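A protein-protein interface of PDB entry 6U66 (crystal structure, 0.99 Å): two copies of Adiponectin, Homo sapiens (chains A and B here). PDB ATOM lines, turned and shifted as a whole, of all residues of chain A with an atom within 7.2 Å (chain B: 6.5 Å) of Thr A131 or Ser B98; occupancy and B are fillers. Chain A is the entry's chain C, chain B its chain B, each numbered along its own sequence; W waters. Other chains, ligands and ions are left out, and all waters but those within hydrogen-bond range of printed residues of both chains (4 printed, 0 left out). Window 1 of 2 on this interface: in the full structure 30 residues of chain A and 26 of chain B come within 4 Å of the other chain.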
ATOM      1  N   SER A  14      32.826 -23.108  22.992  1.00  0.00           N
ATOM      2  CA  SER A  14      31.644 -23.843  23.403  1.00  0.00           C
ATOM      3  C   SER A  14      31.138 -23.140  24.654  1.00  0.00           C
ATOM      4  O   SER A  14      31.878 -23.025  25.654  1.00  0.00           O
ATOM      5  CB  SER A  14      32.003 -25.302  23.603  1.00  0.00           C
ATOM      6  OG  SER A  14      30.863 -26.101  23.924  1.00  0.00           O
ATOM      7  N   VAL A  15      29.897 -22.672  24.610  1.00  0.00           N
ATOM      8  CA  VAL A  15      29.398 -21.735  25.614  1.00  0.00           C
ATOM      9  C   VAL A  15      27.950 -22.089  25.934  1.00  0.00           C
ATOM     10  O   VAL A  15      27.214 -22.664  25.120  1.00  0.00           O
ATOM     11  CB  VAL A  15      29.598 -20.273  25.145  1.00  0.00           C
ATOM     12  CG1 VAL A  15      31.074 -19.917  25.053  1.00  0.00           C
ATOM     13  CG2 VAL A  15      28.878 -19.977  23.816  1.00  0.00           C
ATOM     14  N   GLY A  16      27.522 -21.668  27.130  1.00  0.00           N
ATOM     15  CA  GLY A  16      26.168 -21.914  27.576  1.00  0.00           C
ATOM     16  C   GLY A  16      25.492 -20.683  28.141  1.00  0.00           C
ATOM     17  O   GLY A  16      26.121 -19.740  28.639  1.00  0.00           O
ATOM     18  N   LEU A  17      24.175 -20.714  28.049  1.00  0.00           N
ATOM     19  CA  LEU A  17      23.359 -19.673  28.629  1.00  0.00           C
ATOM     20  C   LEU A  17      23.397 -19.760  30.154  1.00  0.00           C
ATOM     21  O   LEU A  17      23.371 -20.847  30.726  1.00  0.00           O
ATOM     22  CB  LEU A  17      21.934 -19.864  28.106  1.00  0.00           C
ATOM     23  CG  LEU A  17      20.930 -18.781  28.423  1.00  0.00           C
ATOM     24  CD1 LEU A  17      21.330 -17.449  27.741  1.00  0.00           C
ATOM     25  CD2 LEU A  17      19.566 -19.253  27.954  1.00  0.00           C
ATOM     26  N   PHE A  30      25.710 -15.997  25.396  1.00  0.00           N
ATOM     27  CA  PHE A  30      26.080 -17.153  26.191  1.00  0.00           C
ATOM     28  C   PHE A  30      27.339 -16.840  26.980  1.00  0.00           C
ATOM     29  O   PHE A  30      28.331 -16.375  26.387  1.00  0.00           O
ATOM     30  CB  PHE A  30      26.356 -18.358  25.259  1.00  0.00           C
ATOM     31  CG  PHE A  30      25.225 -18.721  24.312  1.00  0.00           C
ATOM     32  CD1 PHE A  30      24.275 -19.672  24.679  1.00  0.00           C
ATOM     33  CD2 PHE A  30      25.116 -18.146  23.066  1.00  0.00           C
ATOM     34  CE1 PHE A  30      23.272 -20.032  23.817  1.00  0.00           C
ATOM     35  CE2 PHE A  30      24.078 -18.484  22.219  1.00  0.00           C
ATOM     36  CZ  PHE A  30      23.143 -19.431  22.598  1.00  0.00           C
ATOM     37  N   LYS A  32      28.536 -18.960  30.017  1.00  0.00           N
ATOM     38  CA  LYS A  32      29.201 -20.106  30.631  1.00  0.00           C
ATOM     39  C   LYS A  32      30.219 -20.619  29.633  1.00  0.00           C
ATOM     40  O   LYS A  32      29.864 -20.945  28.516  1.00  0.00           O
ATOM     41  CB  LYS A  32      28.174 -21.172  30.993  1.00  0.00           C
ATOM     42  CG  LYS A  32      28.699 -22.459  31.674  1.00  0.00           C
ATOM     43  CD  LYS A  32      27.478 -23.395  32.024  1.00  0.00           C
ATOM     44  CE  LYS A  32      27.872 -24.767  32.520  1.00  0.00           C
ATOM     45  NZ  LYS A  32      26.683 -25.742  32.562  1.00  0.00           N
ATOM     46  N   PHE A  34      32.574 -23.316  28.398  1.00  0.00           N
ATOM     47  CA  PHE A  34      33.096 -24.675  28.386  1.00  0.00           C
ATOM     48  C   PHE A  34      34.496 -24.678  27.765  1.00  0.00           C
ATOM     49  O   PHE A  34      35.391 -25.364  28.268  1.00  0.00           O
ATOM     50  CB  PHE A  34      32.167 -25.615  27.613  1.00  0.00           C
ATOM     51  CG  PHE A  34      30.809 -25.749  28.207  1.00  0.00           C
ATOM     52  CD1 PHE A  34      30.605 -26.468  29.386  1.00  0.00           C
ATOM     53  CD2 PHE A  34      29.716 -25.190  27.583  1.00  0.00           C
ATOM     54  CE1 PHE A  34      29.318 -26.629  29.925  1.00  0.00           C
ATOM     55  CE2 PHE A  34      28.454 -25.309  28.130  1.00  0.00           C
ATOM     56  CZ  PHE A  34      28.267 -26.022  29.295  1.00  0.00           C
ATOM     57  N   TYR A  57      32.314 -25.745  11.738  1.00  0.00           N
ATOM     58  CA  TYR A  57      31.095 -26.411  12.181  1.00  0.00           C
ATOM     59  C   TYR A  57      30.504 -25.655  13.350  1.00  0.00           C
ATOM     60  O   TYR A  57      31.233 -25.306  14.287  1.00  0.00           O
ATOM     61  CB  TYR A  57      31.408 -27.848  12.581  1.00  0.00           C
ATOM     62  CG  TYR A  57      30.176 -28.684  12.930  1.00  0.00           C
ATOM     63  CD1 TYR A  57      29.197 -28.951  11.994  1.00  0.00           C
ATOM     64  CD2 TYR A  57      30.043 -29.250  14.181  1.00  0.00           C
ATOM     65  CE1 TYR A  57      28.117 -29.790  12.297  1.00  0.00           C
ATOM     66  CE2 TYR A  57      28.956 -30.067  14.496  1.00  0.00           C
ATOM     67  CZ  TYR A  57      27.986 -30.350  13.558  1.00  0.00           C
ATOM     68  OH  TYR A  57      26.907 -31.132  13.860  1.00  0.00           O
ATOM     69  N   PHE A  58      29.188 -25.434  13.309  1.00  0.00           N
ATOM     70  CA  PHE A  58      28.444 -24.809  14.396  1.00  0.00           C
ATOM     71  C   PHE A  58      27.312 -25.728  14.816  1.00  0.00           C
ATOM     72  O   PHE A  58      26.642 -26.313  13.953  1.00  0.00           O
ATOM     73  CB  PHE A  58      27.848 -23.489  13.944  1.00  0.00           C
ATOM     74  CG  PHE A  58      28.895 -22.452  13.624  1.00  0.00           C
ATOM     75  CD1 PHE A  58      29.466 -21.696  14.661  1.00  0.00           C
ATOM     76  CD2 PHE A  58      29.357 -22.254  12.340  1.00  0.00           C
ATOM     77  CE1 PHE A  58      30.451 -20.771  14.414  1.00  0.00           C
ATOM     78  CE2 PHE A  58      30.352 -21.323  12.068  1.00  0.00           C
ATOM     79  CZ  PHE A  58      30.904 -20.596  13.120  1.00  0.00           C
ATOM     80  N   ALA A  59      27.079 -25.819  16.148  1.00  0.00           N
ATOM     81  CA  ALA A  59      26.020 -26.678  16.673  1.00  0.00           C
ATOM     82  C   ALA A  59      25.445 -26.034  17.930  1.00  0.00           C
ATOM     83  O   ALA A  59      26.212 -25.695  18.854  1.00  0.00           O
ATOM     84  CB  ALA A  59      26.565 -28.056  17.050  1.00  0.00           C
ATOM     85  N   TYR A  60      24.130 -25.956  18.001  1.00  0.00           N
ATOM     86  CA  TYR A  60      23.466 -25.378  19.187  1.00  0.00           C
ATOM     87  C   TYR A  60      22.326 -26.269  19.645  1.00  0.00           C
ATOM     88  O   TYR A  60      21.729 -27.016  18.862  1.00  0.00           O
ATOM     89  CB  TYR A  60      22.985 -23.950  18.901  1.00  0.00           C
ATOM     90  CG  TYR A  60      22.166 -23.790  17.647  1.00  0.00           C
ATOM     91  CD1 TYR A  60      20.775 -23.951  17.633  1.00  0.00           C
ATOM     92  CD2 TYR A  60      22.773 -23.446  16.433  1.00  0.00           C
ATOM     93  CE1 TYR A  60      20.032 -23.785  16.486  1.00  0.00           C
ATOM     94  CE2 TYR A  60      22.045 -23.275  15.283  1.00  0.00           C
ATOM     95  CZ  TYR A  60      20.659 -23.463  15.290  1.00  0.00           C
ATOM     96  OH  TYR A  60      19.953 -23.291  14.106  1.00  0.00           O
ATOM     97  N   HIS A  61      22.044 -26.181  20.948  1.00  0.00           N
ATOM     98  CA  HIS A  61      21.070 -27.009  21.658  1.00  0.00           C
ATOM     99  C   HIS A  61      20.343 -26.112  22.652  1.00  0.00           C
ATOM    100  O   HIS A  61      21.010 -25.432  23.440  1.00  0.00           O
ATOM    101  CB  HIS A  61      21.775 -28.137  22.401  1.00  0.00           C
ATOM    102  CG  HIS A  61      22.523 -29.029  21.478  1.00  0.00           C
ATOM    103  ND1 HIS A  61      21.973 -30.151  20.898  1.00  0.00           N
ATOM    104  CD2 HIS A  61      23.772 -28.924  20.991  1.00  0.00           C
ATOM    105  CE1 HIS A  61      22.870 -30.666  20.073  1.00  0.00           C
ATOM    106  NE2 HIS A  61      23.966 -29.953  20.127  1.00  0.00           N
ATOM    107  N   ILE A  62      19.018 -26.112  22.594  1.00  0.00           N
ATOM    108  CA  ILE A  62      18.216 -25.181  23.381  1.00  0.00           C
ATOM    109  C   ILE A  62      17.170 -25.956  24.159  1.00  0.00           C
ATOM    110  O   ILE A  62      16.361 -26.711  23.584  1.00  0.00           O
ATOM    111  CB  ILE A  62      17.548 -24.144  22.479  1.00  0.00           C
ATOM    112  CG1 ILE A  62      18.620 -23.310  21.750  1.00  0.00           C
ATOM    113  CG2 ILE A  62      16.588 -23.264  23.292  1.00  0.00           C
ATOM    114  CD1 ILE A  62      18.093 -22.415  20.719  1.00  0.00           C
ATOM    115  N   THR A  63      17.128 -25.698  25.475  1.00  0.00           N
ATOM    116  CA  THR A  63      16.021 -26.140  26.308  1.00  0.00           C
ATOM    117  C   THR A  63      14.873 -25.163  26.076  1.00  0.00           C
ATOM    118  O   THR A  63      15.036 -23.945  26.274  1.00  0.00           O
ATOM    119  CB  THR A  63      16.449 -26.157  27.776  1.00  0.00           C
ATOM    120  OG1 THR A  63      17.551 -27.057  27.984  1.00  0.00           O
ATOM    121  CG2 THR A  63      15.283 -26.632  28.635  1.00  0.00           C
ATOM    122  N   ALA A  95      15.541 -28.387  21.281  1.00  0.00           N
ATOM    123  CA  ALA A  95      15.706 -27.975  19.884  1.00  0.00           C
ATOM    124  C   ALA A  95      17.184 -27.856  19.563  1.00  0.00           C
ATOM    125  O   ALA A  95      17.961 -27.350  20.369  1.00  0.00           O
ATOM    126  CB  ALA A  95      15.006 -26.611  19.668  1.00  0.00           C
ATOM    127  N   GLY A  97      20.320 -27.382  16.144  1.00  0.00           N
ATOM    128  CA  GLY A  97      20.705 -27.178  14.762  1.00  0.00           C
ATOM    129  C   GLY A  97      22.199 -27.289  14.628  1.00  0.00           C
ATOM    130  O   GLY A  97      22.939 -27.119  15.602  1.00  0.00           O
ATOM    131  N   SER A  98      22.646 -27.627  13.431  1.00  0.00           N
ATOM    132  CA  SER A  98      24.079 -27.639  13.126  1.00  0.00           C
ATOM    133  C   SER A  98      24.270 -27.489  11.624  1.00  0.00           C
ATOM    134  O   SER A  98      23.444 -27.957  10.842  1.00  0.00           O
ATOM    135  CB  SER A  98      24.819 -28.841  13.683  1.00  0.00           C
ATOM    136  OG  SER A  98      24.609 -30.047  12.923  1.00  0.00           O
ATOM    137  N   LEU A 111      23.912 -16.364  17.244  1.00  0.00           N
ATOM    138  CA  LEU A 111      22.526 -16.772  17.289  1.00  0.00           C
ATOM    139  C   LEU A 111      21.670 -15.610  17.747  1.00  0.00           C
ATOM    140  O   LEU A 111      22.053 -14.878  18.651  1.00  0.00           O
ATOM    141  CB  LEU A 111      22.332 -17.918  18.267  1.00  0.00           C
ATOM    142  CG  LEU A 111      22.697 -19.274  17.745  1.00  0.00           C
ATOM    143  CD1 LEU A 111      22.786 -20.200  18.915  1.00  0.00           C
ATOM    144  CD2 LEU A 111      21.656 -19.790  16.717  1.00  0.00           C
ATOM    145  N   TYR A 123      15.938 -21.587  27.763  1.00  0.00           N
ATOM    146  CA  TYR A 123      15.995 -21.783  29.209  1.00  0.00           C
ATOM    147  C   TYR A 123      17.329 -22.344  29.653  1.00  0.00           C
ATOM    148  O   TYR A 123      17.878 -23.264  29.008  1.00  0.00           O
ATOM    149  CB  TYR A 123      14.889 -22.712  29.706  1.00  0.00           C
ATOM    150  CG  TYR A 123      14.773 -22.743  31.224  1.00  0.00           C
ATOM    151  CD1 TYR A 123      14.290 -21.642  31.936  1.00  0.00           C
ATOM    152  CD2 TYR A 123      15.191 -23.830  31.937  1.00  0.00           C
ATOM    153  CE1 TYR A 123      14.200 -21.658  33.293  1.00  0.00           C
ATOM    154  CE2 TYR A 123      15.130 -23.844  33.332  1.00  0.00           C
ATOM    155  CZ  TYR A 123      14.625 -22.744  33.975  1.00  0.00           C
ATOM    156  OH  TYR A 123      14.524 -22.703  35.361  1.00  0.00           O
ATOM    157  N   ASP A 129      20.669 -26.629  30.497  1.00  0.00           N
ATOM    158  CA  ASP A 129      21.563 -25.869  29.653  1.00  0.00           C
ATOM    159  C   ASP A 129      20.961 -25.587  28.281  1.00  0.00           C
ATOM    160  O   ASP A 129      20.128 -26.331  27.736  1.00  0.00           O
ATOM    161  CB  ASP A 129      22.895 -26.611  29.478  1.00  0.00           C
ATOM    162  CG  ASP A 129      23.787 -26.497  30.716  1.00  0.00           C
ATOM    163  OD1 ASP A 129      24.231 -25.390  31.013  1.00  0.00           O
ATOM    164  OD2 ASP A 129      24.032 -27.520  31.400  1.00  0.00           O
ATOM    165  N   SER A 130      21.444 -24.498  27.695  1.00  0.00           N
ATOM    166  CA  SER A 130      21.238 -24.135  26.280  1.00  0.00           C
ATOM    167  C   SER A 130      22.585 -23.652  25.772  1.00  0.00           C
ATOM    168  O   SER A 130      23.148 -22.715  26.350  1.00  0.00           O
ATOM    169  CB  SER A 130      20.173 -23.059  26.105  1.00  0.00           C
ATOM    170  OG  SER A 130      18.869 -23.497  26.473  1.00  0.00           O
ATOM    171  N   THR A 131      23.129 -24.302  24.718  1.00  0.00           N
ATOM    172  CA  THR A 131      24.517 -24.139  24.343  1.00  0.00           C
ATOM    173  C   THR A 131      24.700 -23.797  22.877  1.00  0.00           C
ATOM    174  O   THR A 131      23.842 -24.021  22.021  1.00  0.00           O
ATOM    175  CB  THR A 131      25.321 -25.432  24.682  1.00  0.00           C
ATOM    176  OG1 THR A 131      24.866 -26.497  23.849  1.00  0.00           O
ATOM    177  CG2 THR A 131      25.154 -25.847  26.146  1.00  0.00           C
ATOM    178  N   PHE A 132      25.883 -23.278  22.591  1.00  0.00           N
ATOM    179  CA  PHE A 132      26.293 -22.867  21.233  1.00  0.00           C
ATOM    180  C   PHE A 132      27.796 -23.190  21.154  1.00  0.00           C
ATOM    181  O   PHE A 132      28.562 -22.768  22.018  1.00  0.00           O
ATOM    182  CB  PHE A 132      26.024 -21.363  21.071  1.00  0.00           C
ATOM    183  CG  PHE A 132      26.401 -20.726  19.782  1.00  0.00           C
ATOM    184  CD1 PHE A 132      26.322 -21.377  18.564  1.00  0.00           C
ATOM    185  CD2 PHE A 132      26.791 -19.387  19.772  1.00  0.00           C
ATOM    186  CE1 PHE A 132      26.641 -20.739  17.345  1.00  0.00           C
ATOM    187  CE2 PHE A 132      27.112 -18.724  18.580  1.00  0.00           C
ATOM    188  CZ  PHE A 132      27.029 -19.418  17.370  1.00  0.00           C
ATOM    189  N   THR A 133      28.174 -23.951  20.108  1.00  0.00           N
ATOM    190  CA  THR A 133      29.538 -24.426  19.907  1.00  0.00           C
ATOM    191  C   THR A 133      29.918 -24.205  18.450  1.00  0.00           C
ATOM    192  O   THR A 133      29.092 -24.369  17.547  1.00  0.00           O
ATOM    193  CB  THR A 133      29.583 -25.946  20.240  1.00  0.00           C
ATOM    194  OG1 THR A 133      29.248 -26.116  21.613  1.00  0.00           O
ATOM    195  CG2 THR A 133      30.910 -26.598  19.943  1.00  0.00           C
ATOM    196  N   TYR B  57      35.142 -33.095  21.157  1.00  0.00           N
ATOM    197  CA  TYR B  57      33.725 -32.825  20.932  1.00  0.00           C
ATOM    198  C   TYR B  57      32.914 -34.026  21.365  1.00  0.00           C
ATOM    199  O   TYR B  57      33.248 -35.156  21.020  1.00  0.00           O
ATOM    200  CB  TYR B  57      33.473 -32.514  19.451  1.00  0.00           C
ATOM    201  CG  TYR B  57      32.031 -32.095  19.122  1.00  0.00           C
ATOM    202  CD1 TYR B  57      31.529 -30.936  19.645  1.00  0.00           C
ATOM    203  CD2 TYR B  57      31.237 -32.815  18.240  1.00  0.00           C
ATOM    204  CE1 TYR B  57      30.247 -30.492  19.319  1.00  0.00           C
ATOM    205  CE2 TYR B  57      29.954 -32.399  17.896  1.00  0.00           C
ATOM    206  CZ  TYR B  57      29.454 -31.219  18.442  1.00  0.00           C
ATOM    207  OH  TYR B  57      28.172 -30.825  18.084  1.00  0.00           O
ATOM    208  N   PHE B  58      31.809 -33.778  22.084  1.00  0.00           N
ATOM    209  CA  PHE B  58      30.864 -34.817  22.517  1.00  0.00           C
ATOM    210  C   PHE B  58      29.475 -34.419  22.051  1.00  0.00           C
ATOM    211  O   PHE B  58      29.096 -33.248  22.154  1.00  0.00           O
ATOM    212  CB  PHE B  58      30.869 -34.981  24.064  1.00  0.00           C
ATOM    213  CG  PHE B  58      32.182 -35.471  24.583  1.00  0.00           C
ATOM    214  CD1 PHE B  58      32.447 -36.830  24.561  1.00  0.00           C
ATOM    215  CD2 PHE B  58      33.181 -34.614  25.025  1.00  0.00           C
ATOM    216  CE1 PHE B  58      33.666 -37.319  24.992  1.00  0.00           C
ATOM    217  CE2 PHE B  58      34.400 -35.093  25.454  1.00  0.00           C
ATOM    218  CZ  PHE B  58      34.643 -36.458  25.436  1.00  0.00           C
ATOM    219  N   ALA B  59      28.716 -35.410  21.574  1.00  0.00           N
ATOM    220  CA  ALA B  59      27.354 -35.167  21.112  1.00  0.00           C
ATOM    221  C   ALA B  59      26.485 -36.389  21.388  1.00  0.00           C
ATOM    222  O   ALA B  59      26.852 -37.504  20.973  1.00  0.00           O
ATOM    223  CB  ALA B  59      27.322 -34.918  19.600  1.00  0.00           C
ATOM    224  N   TYR B  60      25.298 -36.187  21.973  1.00  0.00           N
ATOM    225  CA  TYR B  60      24.384 -37.278  22.285  1.00  0.00           C
ATOM    226  C   TYR B  60      22.985 -36.918  21.783  1.00  0.00           C
ATOM    227  O   TYR B  60      22.594 -35.749  21.739  1.00  0.00           O
ATOM    228  CB  TYR B  60      24.399 -37.631  23.774  1.00  0.00           C
ATOM    229  CG  TYR B  60      24.236 -36.455  24.696  1.00  0.00           C
ATOM    230  CD1 TYR B  60      22.978 -36.043  25.157  1.00  0.00           C
ATOM    231  CD2 TYR B  60      25.343 -35.769  25.181  1.00  0.00           C
ATOM    232  CE1 TYR B  60      22.835 -34.951  26.017  1.00  0.00           C
ATOM    233  CE2 TYR B  60      25.218 -34.696  26.033  1.00  0.00           C
ATOM    234  CZ  TYR B  60      23.965 -34.294  26.465  1.00  0.00           C
ATOM    235  OH  TYR B  60      23.906 -33.231  27.336  1.00  0.00           O
ATOM    236  N   LEU B  73      26.125 -34.825  31.336  1.00  0.00           N
ATOM    237  CA  LEU B  73      27.452 -35.206  30.847  1.00  0.00           C
ATOM    238  C   LEU B  73      28.479 -34.898  31.937  1.00  0.00           C
ATOM    239  O   LEU B  73      28.630 -33.728  32.314  1.00  0.00           O
ATOM    240  CB  LEU B  73      27.803 -34.469  29.551  1.00  0.00           C
ATOM    241  CG  LEU B  73      29.068 -34.947  28.849  1.00  0.00           C
ATOM    242  CD1 LEU B  73      28.876 -36.216  28.090  1.00  0.00           C
ATOM    243  CD2 LEU B  73      29.472 -33.853  27.886  1.00  0.00           C
ATOM    244  N   LEU B  81      27.151 -30.598  32.026  1.00  0.00           N
ATOM    245  CA  LEU B  81      26.144 -30.208  31.058  1.00  0.00           C
ATOM    246  C   LEU B  81      24.885 -31.008  31.363  1.00  0.00           C
ATOM    247  O   LEU B  81      24.981 -32.195  31.685  1.00  0.00           O
ATOM    248  CB  LEU B  81      26.681 -30.539  29.668  1.00  0.00           C
ATOM    249  CG  LEU B  81      25.777 -30.301  28.478  1.00  0.00           C
ATOM    250  CD1 LEU B  81      25.611 -28.833  28.229  1.00  0.00           C
ATOM    251  CD2 LEU B  81      26.364 -31.003  27.230  1.00  0.00           C
ATOM    252  N   THR B  83      20.678 -31.854  30.168  1.00  0.00           N
ATOM    253  CA  THR B  83      19.672 -31.862  29.105  1.00  0.00           C
ATOM    254  C   THR B  83      18.401 -32.515  29.624  1.00  0.00           C
ATOM    255  O   THR B  83      18.444 -33.708  29.949  1.00  0.00           O
ATOM    256  CB  THR B  83      20.189 -32.623  27.859  1.00  0.00           C
ATOM    257  OG1 THR B  83      21.469 -32.119  27.454  1.00  0.00           O
ATOM    258  CG2 THR B  83      19.219 -32.532  26.714  1.00  0.00           C
ATOM    259  N   SER B  96      18.854 -33.676  22.626  1.00  0.00           N
ATOM    260  CA  SER B  96      20.265 -33.762  22.239  1.00  0.00           C
ATOM    261  C   SER B  96      21.058 -32.715  23.006  1.00  0.00           C
ATOM    262  O   SER B  96      20.533 -31.704  23.467  1.00  0.00           O
ATOM    263  CB  SER B  96      20.440 -33.623  20.706  1.00  0.00           C
ATOM    264  OG  SER B  96      20.111 -32.297  20.237  1.00  0.00           O
ATOM    265  N   GLY B  97      22.358 -32.962  23.045  1.00  0.00           N
ATOM    266  CA  GLY B  97      23.316 -32.013  23.600  1.00  0.00           C
ATOM    267  C   GLY B  97      24.667 -32.206  22.942  1.00  0.00           C
ATOM    268  O   GLY B  97      24.963 -33.276  22.410  1.00  0.00           O
ATOM    269  N   SER B  98      25.478 -31.133  22.929  1.00  0.00           N
ATOM    270  CA  SER B  98      26.851 -31.281  22.446  1.00  0.00           C
ATOM    271  C   SER B  98      27.686 -30.139  23.016  1.00  0.00           C
ATOM    272  O   SER B  98      27.174 -29.030  23.227  1.00  0.00           O
ATOM    273  CB  SER B  98      26.958 -31.328  20.919  1.00  0.00           C
ATOM    274  OG  SER B  98      26.780 -30.041  20.303  1.00  0.00           O
ATOM    275  N   VAL B  99      28.979 -30.404  23.214  1.00  0.00           N
ATOM    276  CA  VAL B  99      29.893 -29.445  23.835  1.00  0.00           C
ATOM    277  C   VAL B  99      31.314 -29.819  23.439  1.00  0.00           C
ATOM    278  O   VAL B  99      31.599 -30.997  23.088  1.00  0.00           O
ATOM    279  CB  VAL B  99      29.725 -29.501  25.376  1.00  0.00           C
ATOM    280  CG1 VAL B  99      30.129 -30.853  25.926  1.00  0.00           C
ATOM    281  CG2 VAL B  99      30.459 -28.442  26.123  1.00  0.00           C
ATOM    282  N   LEU B 100      32.215 -28.844  23.534  1.00  0.00           N
ATOM    283  CA  LEU B 100      33.658 -29.076  23.499  1.00  0.00           C
ATOM    284  C   LEU B 100      34.227 -29.052  24.910  1.00  0.00           C
ATOM    285  O   LEU B 100      33.899 -28.140  25.682  1.00  0.00           O
ATOM    286  CB  LEU B 100      34.403 -28.010  22.690  1.00  0.00           C
ATOM    287  CG  LEU B 100      34.109 -27.975  21.168  1.00  0.00           C
ATOM    288  CD1 LEU B 100      34.556 -26.631  20.575  1.00  0.00           C
ATOM    289  CD2 LEU B 100      34.796 -29.110  20.454  1.00  0.00           C
HETATM  290  O   HOH W   1      26.707 -32.258  16.333  1.00  0.00           O
HETATM  291  O   HOH W   2      24.249 -29.165  24.729  1.00  0.00           O
HETATM  292  O   HOH W   3      26.587 -26.841  21.609  1.00  0.00           O
HETATM  293  O   HOH W   4      18.802 -29.899  22.108  1.00  0.00           O
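Hydrophobic or aromatic side chains of chain A that line the printed part of chain B: Phe A34, Tyr A57, Ala A59 and His A61. Among the printed residues, 16 pairs touch across the chains. Among the printed residues, no Asp or Glu carboxylate lies within 4 Å of a Lys or Arg side-chain nitrogen of the other chain.
OG of Ser A14 lies within hydrogen-bond range of N of Leu B100 (3.1 Å). A ring nitrogen (ND1) of His A61 sits at hydrogen-bond distance from the side-chain hydroxyl (OG) of Ser B96. The side-chain hydroxyl of Ser B98 sits at hydrogen-bond distance from a ring nitrogen (NE2) of His A61, at 2.8 Å. The backbone carbonyl oxygen (O) of Ser B98 lies within hydrogen-bond range of the side-chain hydroxyl (OG1) of Thr A131.
Tyr A57 touches its own counterpart, Tyr B57. Ala A59 touches Tyr B57, but with the chains exchanged Tyr A57 does not touch Ala B59 (6.9 Å). Ala A59 touches Ser B98, but with the chains exchanged Ser A98 does not touch Ala B59 (8.7 Å).
Among the printed residues, merely in contact across the chains: Ser A14 with Val B99, Ala A59 with Tyr B57, Phe A34 with Val B99, Asp A129 with Leu B81, His A61 with Gly B97, Phe A34 with Leu B100, Thr A131 with Leu B81, Thr A133 with Leu B100, Tyr A57 with Tyr B57, Ala A59 with Ser B98, Thr A133 with Ser B98 and Thr A133 with Tyr B57.
The side-chain hydroxyl of Thr A133 lies within hydrogen-bond range of the side-chain hydroxyl of Ser A14, at 2.8 Å. The side-chain amino group of Lys A32 is in salt-bridge range of the side-chain carboxylate of Asp A129, at 2.9 Å. The backbone NH of Leu B73 is in hydrogen-bond range of the backbone carbonyl oxygen of Leu B81 (2.9 Å). The backbone carbonyl oxygen (O) of His A61 sits at hydrogen-bond distance from the backbone NH (N) of Thr A131, at 2.7 Å. The side-chain hydroxyl of Ser B98 lies within hydrogen-bond range of the side-chain hydroxyl of Tyr B57 (2.7 Å). OG1 of Thr A63 lies within hydrogen-bond range of O of Asp A129, at 2.7 Å.
Ala A95 touches none of the printed residues of chain B. Thr A131 touches just these residues of chain B: Leu B81 (3.7 Å) and Ser B98 (3.5 Å). Of the printed residues of chain B, Thr A133 touches Tyr B57 (3.999 Å), Ser B98 (3.9 Å) and Leu B100 (3.7 Å). Of the printed residues of chain A, Leu B81 touches Asp A129 (3.4 Å) and Thr A131 (3.7 Å). Of chain A, only Ala A59, His A61, Thr A131 and Thr A133 come within 4 Å of Ser B98. The nearest printed residue of chain B that does not touch Thr A131 is Val B99 (5.7 Å).
Water W1 lies within hydrogen-bond range of OH of Tyr B57 and OH of Tyr A57. Water W3 lies within hydrogen-bond range of the side-chain hydroxyl of Thr A133 (2.8 Å), the backbone carbonyl oxygen of Ser B98 (2.8 Å), the side-chain hydroxyl of Thr A131 (2.8 Å) and the backbone carbonyl oxygen of Ala A59 (3.0 Å). Water W4 lies within hydrogen-bond range of the backbone carbonyl oxygen (O) of Ser B96 (2.8 Å), the backbone carbonyl oxygen (O) of Ala A95 (3.2 Å) and a ring nitrogen (ND1) of His A61 (3.4 Å). Water W2 bridges the side-chain hydroxyl of Thr A131 and the backbone NH of Ser B98.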
